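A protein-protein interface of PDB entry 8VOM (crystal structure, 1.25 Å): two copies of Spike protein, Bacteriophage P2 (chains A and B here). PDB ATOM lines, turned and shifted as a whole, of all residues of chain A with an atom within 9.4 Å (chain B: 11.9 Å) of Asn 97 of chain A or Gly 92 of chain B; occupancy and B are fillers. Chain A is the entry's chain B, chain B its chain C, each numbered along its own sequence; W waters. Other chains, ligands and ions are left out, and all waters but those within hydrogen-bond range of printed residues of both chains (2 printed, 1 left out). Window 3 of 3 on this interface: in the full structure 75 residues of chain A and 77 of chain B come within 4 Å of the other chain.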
ATOM      1  N   GLN A  78       8.428 -20.235 -11.471  1.00  0.00           N
ATOM      2  CA  GLN A  78       9.254 -21.212 -10.775  1.00  0.00           C
ATOM      3  C   GLN A  78      10.147 -22.033 -11.693  1.00  0.00           C
ATOM      4  O   GLN A  78      11.244 -22.435 -11.278  1.00  0.00           O
ATOM      5  CB  GLN A  78       8.342 -22.169 -10.006  1.00  0.00           C
ATOM      6  CG  GLN A  78       7.689 -21.516  -8.801  1.00  0.00           C
ATOM      7  CD  GLN A  78       6.632 -22.380  -8.170  1.00  0.00           C
ATOM      8  OE1 GLN A  78       6.485 -22.387  -6.954  1.00  0.00           O
ATOM      9  NE2 GLN A  78       5.869 -23.100  -8.993  1.00  0.00           N
ATOM     10  N   LYS A  79       9.697 -22.304 -12.923  1.00  0.00           N
ATOM     11  CA  LYS A  79      10.347 -23.277 -13.791  1.00  0.00           C
ATOM     12  C   LYS A  79      10.470 -22.773 -15.225  1.00  0.00           C
ATOM     13  O   LYS A  79      10.453 -23.569 -16.173  1.00  0.00           O
ATOM     14  CB  LYS A  79       9.577 -24.600 -13.787  1.00  0.00           C
ATOM     15  CG  LYS A  79       9.499 -25.262 -12.428  1.00  0.00           C
ATOM     16  CD  LYS A  79       9.033 -26.702 -12.523  1.00  0.00           C
ATOM     17  CE  LYS A  79       9.435 -27.480 -11.283  1.00  0.00           C
ATOM     18  NZ  LYS A  79       9.867 -28.865 -11.617  1.00  0.00           N
ATOM     19  N   GLY A  80      10.589 -21.467 -15.409  1.00  0.00           N
ATOM     20  CA  GLY A  80      10.905 -20.920 -16.709  1.00  0.00           C
ATOM     21  C   GLY A  80       9.689 -20.554 -17.532  1.00  0.00           C
ATOM     22  O   GLY A  80       8.538 -20.561 -17.085  1.00  0.00           O
ATOM     23  N   LEU A  94      16.266  -4.895 -13.480  1.00  0.00           N
ATOM     24  CA  LEU A  94      16.086  -6.239 -14.014  1.00  0.00           C
ATOM     25  C   LEU A  94      17.439  -6.935 -13.941  1.00  0.00           C
ATOM     26  O   LEU A  94      18.406  -6.482 -14.561  1.00  0.00           O
ATOM     27  CB  LEU A  94      15.585  -6.190 -15.457  1.00  0.00           C
ATOM     28  CG  LEU A  94      15.528  -7.508 -16.238  1.00  0.00           C
ATOM     29  CD1 LEU A  94      14.658  -8.551 -15.538  1.00  0.00           C
ATOM     30  CD2 LEU A  94      15.023  -7.261 -17.664  1.00  0.00           C
ATOM     31  N   SER A  95      17.512  -8.012 -13.169  1.00  0.00           N
ATOM     32  CA  SER A  95      18.764  -8.714 -12.944  1.00  0.00           C
ATOM     33  C   SER A  95      18.630 -10.170 -13.368  1.00  0.00           C
ATOM     34  O   SER A  95      17.534 -10.735 -13.362  1.00  0.00           O
ATOM     35  CB  SER A  95      19.167  -8.653 -11.467  1.00  0.00           C
ATOM     36  OG  SER A  95      18.450  -9.613 -10.716  1.00  0.00           O
ATOM     37  N   SER A  96      19.754 -10.773 -13.750  1.00  0.00           N
ATOM     38  CA  SER A  96      19.784 -12.199 -14.042  1.00  0.00           C
ATOM     39  C   SER A  96      21.060 -12.792 -13.467  1.00  0.00           C
ATOM     40  O   SER A  96      22.155 -12.274 -13.710  1.00  0.00           O
ATOM     41  CB  SER A  96      19.710 -12.484 -15.546  1.00  0.00           C
ATOM     42  OG  SER A  96      19.904 -13.868 -15.793  1.00  0.00           O
ATOM     43  N   ASN A  97      20.908 -13.873 -12.703  1.00  0.00           N
ATOM     44  CA  ASN A  97      22.036 -14.544 -12.058  1.00  0.00           C
ATOM     45  C   ASN A  97      22.959 -13.538 -11.375  1.00  0.00           C
ATOM     46  O   ASN A  97      24.187 -13.650 -11.421  1.00  0.00           O
ATOM     47  CB  ASN A  97      22.796 -15.445 -13.033  1.00  0.00           C
ATOM     48  CG  ASN A  97      21.907 -16.502 -13.653  1.00  0.00           C
ATOM     49  OD1 ASN A  97      21.245 -17.266 -12.948  1.00  0.00           O
ATOM     50  ND2 ASN A  97      21.895 -16.562 -14.977  1.00  0.00           N
ATOM     51  N   GLY A  98      22.349 -12.536 -10.744  1.00  0.00           N
ATOM     52  CA  GLY A  98      23.048 -11.612  -9.879  1.00  0.00           C
ATOM     53  C   GLY A  98      23.479 -10.308 -10.510  1.00  0.00           C
ATOM     54  O   GLY A  98      24.004  -9.444  -9.796  1.00  0.00           O
ATOM     55  N   LYS A  99      23.275 -10.129 -11.814  1.00  0.00           N
ATOM     56  CA  LYS A  99      23.782  -8.971 -12.536  1.00  0.00           C
ATOM     57  C   LYS A  99      22.631  -8.125 -13.060  1.00  0.00           C
ATOM     58  O   LYS A  99      21.728  -8.640 -13.726  1.00  0.00           O
ATOM     59  CB  LYS A  99      24.668  -9.413 -13.705  1.00  0.00           C
ATOM     60  CG  LYS A  99      25.819 -10.343 -13.318  1.00  0.00           C
ATOM     61  CD  LYS A  99      26.671  -9.791 -12.173  1.00  0.00           C
ATOM     62  CE  LYS A  99      27.478 -10.897 -11.505  1.00  0.00           C
ATOM     63  NZ  LYS A  99      28.141 -11.770 -12.515  1.00  0.00           N
ATOM     64  N   VAL A 100      22.688  -6.824 -12.781  1.00  0.00           N
ATOM     65  CA  VAL A 100      21.652  -5.890 -13.211  1.00  0.00           C
ATOM     66  C   VAL A 100      21.850  -5.569 -14.687  1.00  0.00           C
ATOM     67  O   VAL A 100      22.866  -4.985 -15.077  1.00  0.00           O
ATOM     68  CB  VAL A 100      21.679  -4.609 -12.365  1.00  0.00           C
ATOM     69  CG1 VAL A 100      20.727  -3.576 -12.950  1.00  0.00           C
ATOM     70  CG2 VAL A 100      21.326  -4.911 -10.913  1.00  0.00           C
ATOM     71  N   LEU A 101      20.871  -5.932 -15.508  1.00  0.00           N
ATOM     72  CA  LEU A 101      20.903  -5.607 -16.927  1.00  0.00           C
ATOM     73  C   LEU A 101      20.506  -4.147 -17.139  1.00  0.00           C
ATOM     74  O   LEU A 101      21.105  -3.441 -17.952  1.00  0.00           O
ATOM     75  CB  LEU A 101      19.960  -6.524 -17.705  1.00  0.00           C
ATOM     76  CG  LEU A 101      20.025  -8.019 -17.380  1.00  0.00           C
ATOM     77  CD1 LEU A 101      19.306  -8.834 -18.450  1.00  0.00           C
ATOM     78  CD2 LEU A 101      21.464  -8.489 -17.237  1.00  0.00           C
ATOM     79  N   ASN B  86      11.532  -4.173  -9.290  1.00  0.00           N
ATOM     80  CA  ASN B  86      12.706  -5.029  -9.383  1.00  0.00           C
ATOM     81  C   ASN B  86      12.302  -6.434  -9.800  1.00  0.00           C
ATOM     82  O   ASN B  86      11.417  -7.041  -9.191  1.00  0.00           O
ATOM     83  CB  ASN B  86      13.467  -5.086  -8.060  1.00  0.00           C
ATOM     84  CG  ASN B  86      13.930  -3.733  -7.614  1.00  0.00           C
ATOM     85  OD1 ASN B  86      14.400  -2.937  -8.427  1.00  0.00           O
ATOM     86  ND2 ASN B  86      13.843  -3.469  -6.315  1.00  0.00           N
ATOM     87  N   ILE B  87      12.955  -6.939 -10.843  1.00  0.00           N
ATOM     88  CA  ILE B  87      12.716  -8.272 -11.381  1.00  0.00           C
ATOM     89  C   ILE B  87      14.032  -9.025 -11.293  1.00  0.00           C
ATOM     90  O   ILE B  87      15.028  -8.612 -11.899  1.00  0.00           O
ATOM     91  CB  ILE B  87      12.206  -8.232 -12.832  1.00  0.00           C
ATOM     92  CG1 ILE B  87      10.964  -7.342 -12.959  1.00  0.00           C
ATOM     93  CG2 ILE B  87      11.930  -9.647 -13.333  1.00  0.00           C
ATOM     94  CD1 ILE B  87       9.679  -7.982 -12.451  1.00  0.00           C
ATOM     95  N   GLU B  88      14.041 -10.114 -10.532  1.00  0.00           N
ATOM     96  CA  GLU B  88      15.242 -10.902 -10.283  1.00  0.00           C
ATOM     97  C   GLU B  88      15.092 -12.256 -10.958  1.00  0.00           C
ATOM     98  O   GLU B  88      14.199 -13.036 -10.612  1.00  0.00           O
ATOM     99  CB  GLU B  88      15.460 -11.079  -8.780  1.00  0.00           C
ATOM    100  CG  GLU B  88      16.531 -12.087  -8.394  1.00  0.00           C
ATOM    101  CD  GLU B  88      16.372 -12.554  -6.957  1.00  0.00           C
ATOM    102  OE1 GLU B  88      16.614 -13.747  -6.678  1.00  0.00           O
ATOM    103  OE2 GLU B  88      15.992 -11.720  -6.108  1.00  0.00           O
ATOM    104  N   HIS B  89      15.981 -12.548 -11.893  1.00  0.00           N
ATOM    105  CA  HIS B  89      16.007 -13.844 -12.543  1.00  0.00           C
ATOM    106  C   HIS B  89      17.204 -14.641 -12.036  1.00  0.00           C
ATOM    107  O   HIS B  89      18.307 -14.101 -11.894  1.00  0.00           O
ATOM    108  CB  HIS B  89      16.093 -13.703 -14.061  1.00  0.00           C
ATOM    109  CG  HIS B  89      16.437 -14.985 -14.741  1.00  0.00           C
ATOM    110  ND1 HIS B  89      17.684 -15.244 -15.266  1.00  0.00           N
ATOM    111  CD2 HIS B  89      15.702 -16.104 -14.940  1.00  0.00           C
ATOM    112  CE1 HIS B  89      17.697 -16.463 -15.774  1.00  0.00           C
ATOM    113  NE2 HIS B  89      16.507 -17.006 -15.589  1.00  0.00           N
ATOM    114  N   THR B  90      16.978 -15.923 -11.751  1.00  0.00           N
ATOM    115  CA  THR B  90      18.054 -16.810 -11.329  1.00  0.00           C
ATOM    116  C   THR B  90      17.782 -18.214 -11.849  1.00  0.00           C
ATOM    117  O   THR B  90      16.708 -18.510 -12.370  1.00  0.00           O
ATOM    118  CB  THR B  90      18.181 -16.871  -9.801  1.00  0.00           C
ATOM    119  OG1 THR B  90      16.955 -17.362  -9.243  1.00  0.00           O
ATOM    120  CG2 THR B  90      18.509 -15.503  -9.218  1.00  0.00           C
ATOM    121  N   GLY B  91      18.777 -19.084 -11.708  1.00  0.00           N
ATOM    122  CA  GLY B  91      18.556 -20.502 -11.935  1.00  0.00           C
ATOM    123  C   GLY B  91      18.296 -20.887 -13.372  1.00  0.00           C
ATOM    124  O   GLY B  91      17.455 -21.755 -13.638  1.00  0.00           O
ATOM    125  N   GLY B  92      19.005 -20.272 -14.305  1.00  0.00           N
ATOM    126  CA  GLY B  92      18.867 -20.607 -15.706  1.00  0.00           C
ATOM    127  C   GLY B  92      19.413 -19.473 -16.547  1.00  0.00           C
ATOM    128  O   GLY B  92      20.172 -18.635 -16.064  1.00  0.00           O
ATOM    129  N   GLU B  93      18.993 -19.457 -17.804  1.00  0.00           N
ATOM    130  CA  GLU B  93      19.447 -18.462 -18.759  1.00  0.00           C
ATOM    131  C   GLU B  93      18.268 -17.632 -19.232  1.00  0.00           C
ATOM    132  O   GLU B  93      17.216 -18.179 -19.574  1.00  0.00           O
ATOM    133  CB  GLU B  93      20.104 -19.140 -19.952  1.00  0.00           C
ATOM    134  CG  GLU B  93      21.600 -19.174 -19.838  1.00  0.00           C
ATOM    135  CD  GLU B  93      22.213 -20.313 -20.618  1.00  0.00           C
ATOM    136  OE1 GLU B  93      21.559 -20.801 -21.567  1.00  0.00           O
ATOM    137  OE2 GLU B  93      23.351 -20.711 -20.285  1.00  0.00           O
ATOM    138  N   LEU B  94      18.449 -16.317 -19.241  1.00  0.00           N
ATOM    139  CA  LEU B  94      17.491 -15.387 -19.827  1.00  0.00           C
ATOM    140  C   LEU B  94      18.034 -15.028 -21.204  1.00  0.00           C
ATOM    141  O   LEU B  94      19.102 -14.418 -21.316  1.00  0.00           O
ATOM    142  CB  LEU B  94      17.348 -14.144 -18.951  1.00  0.00           C
ATOM    143  CG  LEU B  94      16.445 -13.013 -19.454  1.00  0.00           C
ATOM    144  CD1 LEU B  94      15.001 -13.457 -19.603  1.00  0.00           C
ATOM    145  CD2 LEU B  94      16.531 -11.800 -18.526  1.00  0.00           C
ATOM    146  N   SER B  95      17.320 -15.430 -22.249  1.00  0.00           N
ATOM    147  CA  SER B  95      17.747 -15.206 -23.622  1.00  0.00           C
ATOM    148  C   SER B  95      16.711 -14.362 -24.350  1.00  0.00           C
ATOM    149  O   SER B  95      15.509 -14.586 -24.211  1.00  0.00           O
ATOM    150  CB  SER B  95      17.922 -16.543 -24.347  1.00  0.00           C
ATOM    151  OG  SER B  95      16.682 -17.212 -24.485  1.00  0.00           O
ATOM    152  N   SER B  96      17.174 -13.378 -25.115  1.00  0.00           N
ATOM    153  CA  SER B  96      16.284 -12.560 -25.928  1.00  0.00           C
ATOM    154  C   SER B  96      16.776 -12.614 -27.364  1.00  0.00           C
ATOM    155  O   SER B  96      17.960 -12.375 -27.626  1.00  0.00           O
ATOM    156  CB  SER B  96      16.226 -11.109 -25.434  1.00  0.00           C
ATOM    157  OG  SER B  96      15.476 -10.287 -26.317  1.00  0.00           O
ATOM    158  N   LYS B  99      20.132 -14.406 -27.941  1.00  0.00           N
ATOM    159  CA  LYS B  99      21.301 -14.053 -27.149  1.00  0.00           C
ATOM    160  C   LYS B  99      21.030 -14.370 -25.684  1.00  0.00           C
ATOM    161  O   LYS B  99      20.070 -13.854 -25.102  1.00  0.00           O
ATOM    162  CB  LYS B  99      21.610 -12.561 -27.289  1.00  0.00           C
ATOM    163  CG  LYS B  99      22.831 -12.083 -26.492  1.00  0.00           C
ATOM    164  CD  LYS B  99      23.038 -10.554 -26.532  1.00  0.00           C
ATOM    165  CE  LYS B  99      22.950  -9.941 -27.936  1.00  0.00           C
ATOM    166  NZ  LYS B  99      22.440  -8.533 -27.901  1.00  0.00           N
ATOM    167  N   VAL B 100      21.878 -15.206 -25.090  1.00  0.00           N
ATOM    168  CA  VAL B 100      21.882 -15.352 -23.640  1.00  0.00           C
ATOM    169  C   VAL B 100      22.403 -14.053 -23.039  1.00  0.00           C
ATOM    170  O   VAL B 100      23.498 -13.591 -23.380  1.00  0.00           O
ATOM    171  CB  VAL B 100      22.734 -16.555 -23.217  1.00  0.00           C
ATOM    172  CG1 VAL B 100      22.954 -16.547 -21.713  1.00  0.00           C
ATOM    173  CG2 VAL B 100      22.066 -17.850 -23.656  1.00  0.00           C
ATOM    174  N   LEU B 101      21.617 -13.454 -22.152  1.00  0.00           N
ATOM    175  CA  LEU B 101      21.976 -12.172 -21.557  1.00  0.00           C
ATOM    176  C   LEU B 101      22.678 -12.376 -20.218  1.00  0.00           C
ATOM    177  O   LEU B 101      23.364 -11.480 -19.728  1.00  0.00           O
ATOM    178  CB  LEU B 101      20.727 -11.306 -21.369  1.00  0.00           C
ATOM    179  CG  LEU B 101      19.773 -11.232 -22.566  1.00  0.00           C
ATOM    180  CD1 LEU B 101      18.554 -10.378 -22.228  1.00  0.00           C
ATOM    181  CD2 LEU B 101      20.471 -10.703 -23.815  1.00  0.00           C
HETATM  182  O   HOH W   1      20.883 -15.148 -18.240  1.00  0.00           O
HETATM  183  O   HOH W   2      16.589  -6.834  -9.762  1.00  0.00           O
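N of Ser 95 of chain A sits at hydrogen-bond distance from O of Ile 87 of chain B, at 2.9 Å. The backbone NH (N) of His 89 of chain B lies within hydrogen-bond range of the backbone carbonyl oxygen (O) of Ser 95 of chain A (2.8 Å). The side-chain hydroxyl (OG) of Ser 96 of chain A lies within hydrogen-bond range of a ring nitrogen (ND1) of His 89 of chain B. N of Asn 97 of chain A is in hydrogen-bond range of O of His 89 of chain B. The side-chain amide oxygen (OD1) of Asn 97 of chain A is in hydrogen-bond range of the backbone NH (N) of Gly 91 of chain B. The side-chain amide nitrogen (ND2) of Asn 97 of chain A is in hydrogen-bond range of the backbone carbonyl oxygen (O) of Gly 92 of chain B (2.9 Å).
The backbone NH of Leu 101 of chain A sits at hydrogen-bond distance from the backbone carbonyl oxygen of Leu 94 of chain A (2.7 Å). The side-chain amide nitrogen of Asn 97 of chain A is in hydrogen-bond range of the side-chain hydroxyl of Ser 96 of chain A, 3.4 Å away.
O of Ile 87 of chain B touches CA of Leu 94 of chain A, at 3.4 Å. Ser 95 of chain A touches Glu 88 of chain B (OG to CA, 3.5 Å). Thr 90 of chain B touches Asn 97 of chain A (CA to OD1, 3.6 Å).
Of the printed residues of chain B, Leu 94 of chain A touches Ile 87. Of chain B, only His 89 (2.7 Å), Thr 90 (3.6 Å), Gly 91 (3.3 Å) and Gly 92 (2.9 Å) come within 4 Å of Asn 97 of chain A. No residue of chain B comes within 4 Å of Gly 98 of chain A. No residue of chain B comes within 4 Å of Lys 99 of chain A. Of the printed residues of chain A, Ile 87 of chain B touches Leu 94 (3.4 Å) and Ser 95 (2.9 Å). Of the printed residues of chain A, Glu 88 of chain B touches Ser 95 (3.5 Å). His 89 of chain B touches just these residues of chain A: Ser 95 (2.8 Å), Ser 96 (2.7 Å) and Asn 97 (2.7 Å). Of the printed residues of chain A, Thr 90 of chain B touches Asn 97 (3.6 Å). Gly 92 of chain B touches just one residue of chain A: Asn 97 (2.9 Å). The nearest residue of chain A that does not touch Gly 92 of chain B is Ser 96 of chain A (4.8 Å).
Of the 14 printed residues of chain B, 6 touch a printed residue of chain A. Hydrophobic or aromatic side chains of chain B within 4 Å of the printed part of chain A: Ile 87 and His 89. Along chain B the printed residues that touch a printed residue of chain A span positions 87 to 92. Of the 11 printed residues of chain A, 4 touch a printed residue of chain B. Hydrophobic or aromatic side chains of chain A that line the printed part of chain B: Leu 94. Along chain A the printed residues that touch a printed residue of chain B span positions 94 to 97. Among the printed residues, 9 pairs touch across the chains. Among the printed residues, no Asp or Glu carboxylate lies within 4 Å of a Lys or Arg side-chain nitrogen of the other chain.
6 positions are printed for both chains. Of the 9 pairs that touch across the chains among the printed residues, none has its exchanged pair printed and touching as well.
Water W1 lies within hydrogen-bond range of N of Leu 94 of chain B (2.9 Å) and OG of Ser 96 of chain A (2.9 Å). Water W2 lies within hydrogen-bond range of the backbone carbonyl oxygen of Ile 87 of chain B (3.2 Å) and the side-chain hydroxyl of Ser 95 of chain A (3.5 Å).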
